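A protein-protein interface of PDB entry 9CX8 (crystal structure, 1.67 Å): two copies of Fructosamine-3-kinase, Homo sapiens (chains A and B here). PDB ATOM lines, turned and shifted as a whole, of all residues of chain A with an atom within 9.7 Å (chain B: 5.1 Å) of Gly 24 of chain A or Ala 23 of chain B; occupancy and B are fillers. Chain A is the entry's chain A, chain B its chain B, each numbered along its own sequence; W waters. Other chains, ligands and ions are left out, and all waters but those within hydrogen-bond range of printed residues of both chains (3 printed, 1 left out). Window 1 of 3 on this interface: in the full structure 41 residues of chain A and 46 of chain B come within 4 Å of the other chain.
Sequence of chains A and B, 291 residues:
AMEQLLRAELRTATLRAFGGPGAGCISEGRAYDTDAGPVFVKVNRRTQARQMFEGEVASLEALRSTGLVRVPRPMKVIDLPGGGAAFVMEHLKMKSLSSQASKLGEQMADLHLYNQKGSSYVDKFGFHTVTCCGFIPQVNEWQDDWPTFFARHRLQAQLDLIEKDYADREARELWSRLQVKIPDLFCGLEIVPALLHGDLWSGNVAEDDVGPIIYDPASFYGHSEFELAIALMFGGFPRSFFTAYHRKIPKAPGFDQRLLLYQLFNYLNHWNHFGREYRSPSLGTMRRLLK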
ATOM      1  N   GLY A  19      11.838   2.289 -15.994  1.00  0.00           N
ATOM      2  CA  GLY A  19      11.340   0.926 -16.070  1.00  0.00           C
ATOM      3  C   GLY A  19      12.370  -0.158 -15.754  1.00  0.00           C
ATOM      4  O   GLY A  19      13.587   0.052 -15.745  1.00  0.00           O
ATOM      5  N   GLY A  20      11.819  -1.375 -15.543  1.00  0.00           N
ATOM      6  CA  GLY A  20      12.558  -2.532 -15.071  1.00  0.00           C
ATOM      7  C   GLY A  20      13.295  -3.243 -16.187  1.00  0.00           C
ATOM      8  O   GLY A  20      13.146  -2.936 -17.385  1.00  0.00           O
ATOM      9  N   PRO A  21      14.110  -4.235 -15.801  1.00  0.00           N
ATOM     10  CA  PRO A  21      15.069  -4.802 -16.766  1.00  0.00           C
ATOM     11  C   PRO A  21      14.442  -5.701 -17.827  1.00  0.00           C
ATOM     12  O   PRO A  21      15.026  -5.836 -18.909  1.00  0.00           O
ATOM     13  CB  PRO A  21      16.038  -5.588 -15.868  1.00  0.00           C
ATOM     14  CG  PRO A  21      15.185  -6.021 -14.693  1.00  0.00           C
ATOM     15  CD  PRO A  21      14.250  -4.844 -14.457  1.00  0.00           C
ATOM     16  N   GLY A  22      13.294  -6.331 -17.559  1.00  0.00           N
ATOM     17  CA  GLY A  22      12.753  -7.304 -18.491  1.00  0.00           C
ATOM     18  C   GLY A  22      13.238  -8.723 -18.244  1.00  0.00           C
ATOM     19  O   GLY A  22      13.887  -9.059 -17.243  1.00  0.00           O
ATOM     20  N   ALA A  23      12.927  -9.577 -19.228  1.00  0.00           N
ATOM     21  CA  ALA A  23      13.140 -11.010 -19.103  1.00  0.00           C
ATOM     22  C   ALA A  23      14.618 -11.397 -19.117  1.00  0.00           C
ATOM     23  O   ALA A  23      14.963 -12.458 -18.607  1.00  0.00           O
ATOM     24  CB  ALA A  23      12.381 -11.726 -20.231  1.00  0.00           C
ATOM     25  N   GLY A  24      15.482 -10.580 -19.704  1.00  0.00           N
ATOM     26  CA  GLY A  24      16.907 -10.800 -19.635  1.00  0.00           C
ATOM     27  C   GLY A  24      17.444 -11.593 -20.805  1.00  0.00           C
ATOM     28  O   GLY A  24      16.910 -11.549 -21.921  1.00  0.00           O
ATOM     29  N   CYS A  25      18.485 -12.362 -20.523  1.00  0.00           N
ATOM     30  CA  CYS A  25      19.304 -13.031 -21.522  1.00  0.00           C
ATOM     31  C   CYS A  25      19.139 -14.530 -21.328  1.00  0.00           C
ATOM     32  O   CYS A  25      19.499 -15.068 -20.274  1.00  0.00           O
ATOM     33  CB  CYS A  25      20.769 -12.611 -21.375  1.00  0.00           C
ATOM     34  SG  CYS A  25      21.971 -13.606 -22.405  1.00  0.00           S
ATOM     35  N   ILE A  26      18.594 -15.187 -22.358  1.00  0.00           N
ATOM     36  CA  ILE A  26      18.201 -16.595 -22.298  1.00  0.00           C
ATOM     37  C   ILE A  26      19.381 -17.469 -21.886  1.00  0.00           C
ATOM     38  O   ILE A  26      19.234 -18.406 -21.092  1.00  0.00           O
ATOM     39  CB  ILE A  26      17.597 -17.025 -23.668  1.00  0.00           C
ATOM     40  CG1 ILE A  26      16.910 -18.396 -23.590  1.00  0.00           C
ATOM     41  CG2 ILE A  26      18.685 -17.045 -24.833  1.00  0.00           C
ATOM     42  CD1 ILE A  26      16.119 -18.769 -24.888  1.00  0.00           C
ATOM     43  N   SER A  27      20.575 -17.149 -22.378  1.00  0.00           N
ATOM     44  CA  SER A  27      21.732 -17.985 -22.112  1.00  0.00           C
ATOM     45  C   SER A  27      22.336 -17.734 -20.737  1.00  0.00           C
ATOM     46  O   SER A  27      23.213 -18.496 -20.306  1.00  0.00           O
ATOM     47  CB  SER A  27      22.828 -17.743 -23.163  1.00  0.00           C
ATOM     48  OG  SER A  27      23.489 -16.497 -22.919  1.00  0.00           O
ATOM     49  N   GLU A  28      21.909 -16.698 -20.034  1.00  0.00           N
ATOM     50  CA  GLU A  28      22.529 -16.400 -18.742  1.00  0.00           C
ATOM     51  C   GLU A  28      21.726 -16.915 -17.563  1.00  0.00           C
ATOM     52  O   GLU A  28      22.311 -17.262 -16.539  1.00  0.00           O
ATOM     53  CB  GLU A  28      22.732 -14.896 -18.576  1.00  0.00           C
ATOM     54  CG  GLU A  28      23.843 -14.351 -19.495  1.00  0.00           C
ATOM     55  CD  GLU A  28      24.113 -12.877 -19.253  1.00  0.00           C
ATOM     56  OE1 GLU A  28      25.263 -12.433 -19.480  1.00  0.00           O
ATOM     57  OE2 GLU A  28      23.156 -12.160 -18.864  1.00  0.00           O
ATOM     58  N   GLY A  29      20.418 -16.975 -17.679  1.00  0.00           N
ATOM     59  CA  GLY A  29      19.591 -17.351 -16.561  1.00  0.00           C
ATOM     60  C   GLY A  29      18.399 -16.429 -16.478  1.00  0.00           C
ATOM     61  O   GLY A  29      18.171 -15.593 -17.353  1.00  0.00           O
ATOM     62  N   ARG A  30      17.606 -16.580 -15.413  1.00  0.00           N
ATOM     63  CA  ARG A  30      16.324 -15.867 -15.309  1.00  0.00           C
ATOM     64  C   ARG A  30      16.095 -15.401 -13.886  1.00  0.00           C
ATOM     65  O   ARG A  30      16.415 -16.128 -12.944  1.00  0.00           O
ATOM     66  CB  ARG A  30      15.136 -16.762 -15.729  1.00  0.00           C
ATOM     67  CG  ARG A  30      13.767 -16.029 -15.993  1.00  0.00           C
ATOM     68  CD  ARG A  30      13.655 -15.376 -17.415  1.00  0.00           C
ATOM     69  NE  ARG A  30      12.356 -14.744 -17.672  1.00  0.00           N
ATOM     70  CZ  ARG A  30      11.447 -15.239 -18.514  1.00  0.00           C
ATOM     71  NH1 ARG A  30      11.669 -16.365 -19.168  1.00  0.00           N
ATOM     72  NH2 ARG A  30      10.283 -14.593 -18.686  1.00  0.00           N
ATOM     73  N   ALA A  31      15.581 -14.181 -13.739  1.00  0.00           N
ATOM     74  CA  ALA A  31      15.222 -13.608 -12.451  1.00  0.00           C
ATOM     75  C   ALA A  31      13.768 -13.870 -12.127  1.00  0.00           C
ATOM     76  O   ALA A  31      12.896 -13.854 -13.013  1.00  0.00           O
ATOM     77  CB  ALA A  31      15.434 -12.095 -12.428  1.00  0.00           C
ATOM     78  N   PHE A  40      18.052 -14.812  -8.811  1.00  0.00           N
ATOM     79  CA  PHE A  40      18.481 -15.124 -10.171  1.00  0.00           C
ATOM     80  C   PHE A  40      18.852 -16.589 -10.225  1.00  0.00           C
ATOM     81  O   PHE A  40      19.560 -17.079  -9.341  1.00  0.00           O
ATOM     82  CB  PHE A  40      19.698 -14.246 -10.565  1.00  0.00           C
ATOM     83  CG  PHE A  40      20.057 -14.342 -12.051  1.00  0.00           C
ATOM     84  CD1 PHE A  40      19.350 -13.598 -12.976  1.00  0.00           C
ATOM     85  CD2 PHE A  40      21.071 -15.187 -12.506  1.00  0.00           C
ATOM     86  CE1 PHE A  40      19.629 -13.701 -14.323  1.00  0.00           C
ATOM     87  CE2 PHE A  40      21.365 -15.258 -13.836  1.00  0.00           C
ATOM     88  CZ  PHE A  40      20.630 -14.518 -14.757  1.00  0.00           C
ATOM     89  N   HIS A  91      19.237 -11.616  -6.306  1.00  0.00           N
ATOM     90  CA  HIS A  91      19.236 -10.745  -7.473  1.00  0.00           C
ATOM     91  C   HIS A  91      19.195  -9.294  -7.008  1.00  0.00           C
ATOM     92  O   HIS A  91      18.402  -8.941  -6.140  1.00  0.00           O
ATOM     93  CB  HIS A  91      18.035 -11.008  -8.390  1.00  0.00           C
ATOM     94  CG  HIS A  91      18.072 -10.198  -9.648  1.00  0.00           C
ATOM     95  ND1 HIS A  91      19.031 -10.384 -10.629  1.00  0.00           N
ATOM     96  CD2 HIS A  91      17.293  -9.174 -10.067  1.00  0.00           C
ATOM     97  CE1 HIS A  91      18.806  -9.541 -11.619  1.00  0.00           C
ATOM     98  NE2 HIS A  91      17.766  -8.792 -11.299  1.00  0.00           N
ATOM     99  N   MET A  94      19.915  -3.473 -10.643  1.00  0.00           N
ATOM    100  CA  MET A  94      21.235  -2.995 -11.060  1.00  0.00           C
ATOM    101  C   MET A  94      21.160  -2.225 -12.372  1.00  0.00           C
ATOM    102  O   MET A  94      20.363  -2.554 -13.257  1.00  0.00           O
ATOM    103  CB  MET A  94      22.183  -4.157 -11.329  1.00  0.00           C
ATOM    104  CG  MET A  94      22.247  -5.227 -10.292  1.00  0.00           C
ATOM    105  SD  MET A  94      23.672  -6.307 -10.634  1.00  0.00           S
ATOM    106  CE  MET A  94      23.143  -7.049 -12.150  1.00  0.00           C
ATOM    107  N   LYS A  95      22.084  -1.280 -12.538  1.00  0.00           N
ATOM    108  CA  LYS A  95      22.265  -0.508 -13.768  1.00  0.00           C
ATOM    109  C   LYS A  95      23.737  -0.574 -14.177  1.00  0.00           C
ATOM    110  O   LYS A  95      24.592  -1.011 -13.400  1.00  0.00           O
ATOM    111  CB  LYS A  95      21.821   0.950 -13.565  1.00  0.00           C
ATOM    112  N   SER A  96      24.036  -0.131 -15.401  1.00  0.00           N
ATOM    113  CA  SER A  96      25.406  -0.126 -15.896  1.00  0.00           C
ATOM    114  C   SER A  96      26.327   0.645 -14.962  1.00  0.00           C
ATOM    115  O   SER A  96      25.941   1.645 -14.355  1.00  0.00           O
ATOM    116  CB  SER A  96      25.481   0.512 -17.286  1.00  0.00           C
ATOM    117  OG  SER A  96      25.042  -0.419 -18.253  1.00  0.00           O
ATOM    118  N   GLY B  20       8.754  -9.226 -19.908  1.00  0.00           N
ATOM    119  CA  GLY B  20       8.894  -8.082 -20.768  1.00  0.00           C
ATOM    120  C   GLY B  20      10.231  -7.961 -21.477  1.00  0.00           C
ATOM    121  O   GLY B  20      11.221  -8.641 -21.152  1.00  0.00           O
ATOM    122  N   PRO B  21      10.258  -7.069 -22.489  1.00  0.00           N
ATOM    123  CA  PRO B  21      11.491  -6.816 -23.246  1.00  0.00           C
ATOM    124  C   PRO B  21      12.450  -5.996 -22.408  1.00  0.00           C
ATOM    125  O   PRO B  21      12.099  -5.445 -21.360  1.00  0.00           O
ATOM    126  CB  PRO B  21      11.047  -6.020 -24.482  1.00  0.00           C
ATOM    127  CG  PRO B  21       9.661  -5.456 -24.146  1.00  0.00           C
ATOM    128  CD  PRO B  21       9.116  -6.244 -22.932  1.00  0.00           C
ATOM    129  N   GLY B  22      13.675  -5.908 -22.918  1.00  0.00           N
ATOM    130  CA  GLY B  22      14.736  -5.163 -22.262  1.00  0.00           C
ATOM    131  C   GLY B  22      16.059  -5.536 -22.897  1.00  0.00           C
ATOM    132  O   GLY B  22      16.097  -6.013 -24.039  1.00  0.00           O
ATOM    133  N   ALA B  23      17.142  -5.336 -22.143  1.00  0.00           N
ATOM    134  CA  ALA B  23      18.445  -5.789 -22.606  1.00  0.00           C
ATOM    135  C   ALA B  23      18.473  -7.322 -22.621  1.00  0.00           C
ATOM    136  O   ALA B  23      18.248  -7.970 -21.589  1.00  0.00           O
ATOM    137  CB  ALA B  23      19.545  -5.222 -21.711  1.00  0.00           C
ATOM    138  N   GLY B  24      18.700  -7.896 -23.795  1.00  0.00           N
ATOM    139  CA  GLY B  24      18.818  -9.336 -23.975  1.00  0.00           C
ATOM    140  C   GLY B  24      20.265  -9.762 -24.112  1.00  0.00           C
ATOM    141  O   GLY B  24      21.185  -9.102 -23.607  1.00  0.00           O
ATOM    142  N   CYS B  25      20.477 -10.895 -24.786  1.00  0.00           N
ATOM    143  CA  CYS B  25      21.845 -11.342 -25.020  1.00  0.00           C
ATOM    144  C   CYS B  25      22.501 -10.592 -26.159  1.00  0.00           C
ATOM    145  O   CYS B  25      23.737 -10.533 -26.201  1.00  0.00           O
ATOM    146  CB  CYS B  25      21.903 -12.826 -25.367  1.00  0.00           C
ATOM    147  SG  CYS B  25      21.081 -13.905 -24.220  1.00  0.00           S
ATOM    148  N   SER B  27      20.886  -7.438 -28.029  1.00  0.00           N
ATOM    149  CA  SER B  27      20.720  -5.986 -28.110  1.00  0.00           C
ATOM    150  C   SER B  27      20.404  -5.367 -26.738  1.00  0.00           C
ATOM    151  O   SER B  27      19.806  -5.993 -25.871  1.00  0.00           O
ATOM    152  CB  SER B  27      19.612  -5.602 -29.120  1.00  0.00           C
ATOM    153  OG  SER B  27      19.896  -6.091 -30.447  1.00  0.00           O
ATOM    154  N   GLU B  28      20.795  -4.111 -26.572  1.00  0.00           N
ATOM    155  CA  GLU B  28      20.375  -3.303 -25.433  1.00  0.00           C
ATOM    156  C   GLU B  28      18.917  -2.900 -25.615  1.00  0.00           C
ATOM    157  O   GLU B  28      18.420  -2.822 -26.738  1.00  0.00           O
ATOM    158  CB  GLU B  28      21.235  -2.034 -25.332  1.00  0.00           C
ATOM    159  CG  GLU B  28      22.752  -2.231 -25.120  1.00  0.00           C
ATOM    160  CD  GLU B  28      23.614  -1.127 -25.821  1.00  0.00           C
ATOM    161  OE1 GLU B  28      24.641  -1.467 -26.465  1.00  0.00           O
ATOM    162  OE2 GLU B  28      23.298   0.087 -25.674  1.00  0.00           O
ATOM    163  N   GLY B  29      18.215  -2.655 -24.511  1.00  0.00           N
ATOM    164  CA  GLY B  29      16.827  -2.216 -24.635  1.00  0.00           C
ATOM    165  C   GLY B  29      16.369  -1.383 -23.453  1.00  0.00           C
ATOM    166  O   GLY B  29      16.590  -1.774 -22.301  1.00  0.00           O
ATOM    167  N   TRP B 201      10.088 -17.968 -27.193  1.00  0.00           N
ATOM    168  CA  TRP B 201      10.627 -18.168 -25.859  1.00  0.00           C
ATOM    169  C   TRP B 201       9.707 -17.535 -24.813  1.00  0.00           C
ATOM    170  O   TRP B 201       9.060 -16.519 -25.070  1.00  0.00           O
ATOM    171  CB  TRP B 201      12.046 -17.500 -25.839  1.00  0.00           C
ATOM    172  CG  TRP B 201      12.694 -17.328 -24.481  1.00  0.00           C
ATOM    173  CD1 TRP B 201      12.852 -18.311 -23.486  1.00  0.00           C
ATOM    174  CD2 TRP B 201      13.392 -16.181 -24.026  1.00  0.00           C
ATOM    175  NE1 TRP B 201      13.550 -17.774 -22.405  1.00  0.00           N
ATOM    176  CE2 TRP B 201      13.884 -16.473 -22.699  1.00  0.00           C
ATOM    177  CE3 TRP B 201      13.560 -14.914 -24.548  1.00  0.00           C
ATOM    178  CZ2 TRP B 201      14.564 -15.538 -21.926  1.00  0.00           C
ATOM    179  CZ3 TRP B 201      14.270 -13.961 -23.750  1.00  0.00           C
ATOM    180  CH2 TRP B 201      14.734 -14.289 -22.449  1.00  0.00           C
HETATM  181  O   HOH W   1      16.812  -3.827 -19.648  1.00  0.00           O
HETATM  182  O   HOH W   2      17.619 -13.268 -24.654  1.00  0.00           O
HETATM  183  O   HOH W   3      14.086 -18.535 -19.496  1.00  0.00           O
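N of Ala 23 of chain A sits at hydrogen-bond distance from O of Gly 20 of chain B (2.7 Å). SG of Cys 25 of chain A is disulfide-bonded to SG of Cys 25 of chain B (2.0 Å). The backbone NH of Ser 27 of chain A lies within hydrogen-bond range of the side-chain sulfur of Cys 25 of chain B. N of Ile 26 of chain A is in hydrogen-bond range of SG of Cys 25 of chain B (3.4 Å).
The side-chain hydroxyl of Ser 27 of chain A lies within hydrogen-bond range of the side-chain sulfur of Cys 25 of chain A (3.3 Å).
Among the printed residues, merely in contact across the chains: Pro 21 of chain A with Pro 21 of chain B (3.8 Å), Pro 21 of chain A with Gly 22 of chain B (3.4 Å), Pro 21 of chain A with Ala 23 of chain B (3.9 Å), Gly 22 of chain A with Gly 20 of chain B (3.3 Å), Gly 22 of chain A with Pro 21 of chain B (3.5 Å), Gly 24 of chain A with Ala 23 of chain B (3.7 Å), Gly 24 of chain A with Gly 24 of chain B (3.6 Å), Gly 24 of chain A with Trp 201 of chain B (3.5 Å), Cys 25 of chain A with Gly 24 of chain B (3.98 Å) and Ile 26 of chain A with Trp 201 of chain B (3.6 Å).
Of chain B, only Ala 23, Gly 24 and Trp 201 come within 4 Å of Gly 24 of chain A. Ala 23 of chain B touches just these residues of chain A: Pro 21 and Gly 24. No residue of chain A comes within 4 Å of Gly 29 of chain B. Printed residues of chain A within 4 Å of Gly 20 of chain B: Gly 22 (3.3 Å) and Ala 23 (2.7 Å). Of the printed residues of chain A, Pro 21 of chain B touches Pro 21 and Gly 22. Gly 20 of chain A touches none of the printed residues of chain B. The nearest residue of chain B that does not touch Gly 24 of chain A is Cys 25 of chain B (4.6 Å). The nearest residue of chain A that does not touch Ala 23 of chain B is Cys 25 of chain A (4.5 Å). The nearest printed residue of chain B that does not touch Ser 27 of chain A is Trp 201 of chain B (6.2 Å).
Hydrophobic or aromatic side chains of chain A that line the printed part of chain B: Ala 23 and Ile 26. Among the printed residues, 14 pairs touch across the chains. Among the printed residues, no Asp or Glu carboxylate lies within 4 Å of a Lys or Arg side-chain nitrogen of the other chain.
Ala 23 of chain A touches Gly 20 of chain B, but with the chains exchanged Gly 20 of chain A does not touch Ala 23 of chain B (6.7 Å). Gly 24 of chain A touches its own counterpart, Gly 24 of chain B. Cys 25 of chain A touches Gly 24 of chain B, but with the chains exchanged Gly 24 of chain A does not touch Cys 25 of chain B (4.6 Å). Cys 25 of chain A touches its own counterpart, Cys 25 of chain B. Of the 14 pairs that touch across the chains among the printed residues, 5 have their exchanged pair printed and touching as well.
Water W1 lies within hydrogen-bond range of the backbone carbonyl oxygen (O) of Pro 21 of chain A (2.8 Å), the backbone NH (N) of Ala 23 of chain B (2.9 Å) and the backbone carbonyl oxygen (O) of Gly 29 of chain B (3.4 Å). Water W3 bridges the indole nitrogen (NE1) of Trp 201 of chain B (3.1 Å) and the guanidinium group (NH1) of Arg 30 of chain A (3.3 Å). Water W2 lies within hydrogen-bond range of the backbone NH (N) of Ile 26 of chain A, the backbone carbonyl oxygen (O) of Gly 24 of chain A and the side-chain sulfur (SG) of Cys 25 of chain B.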
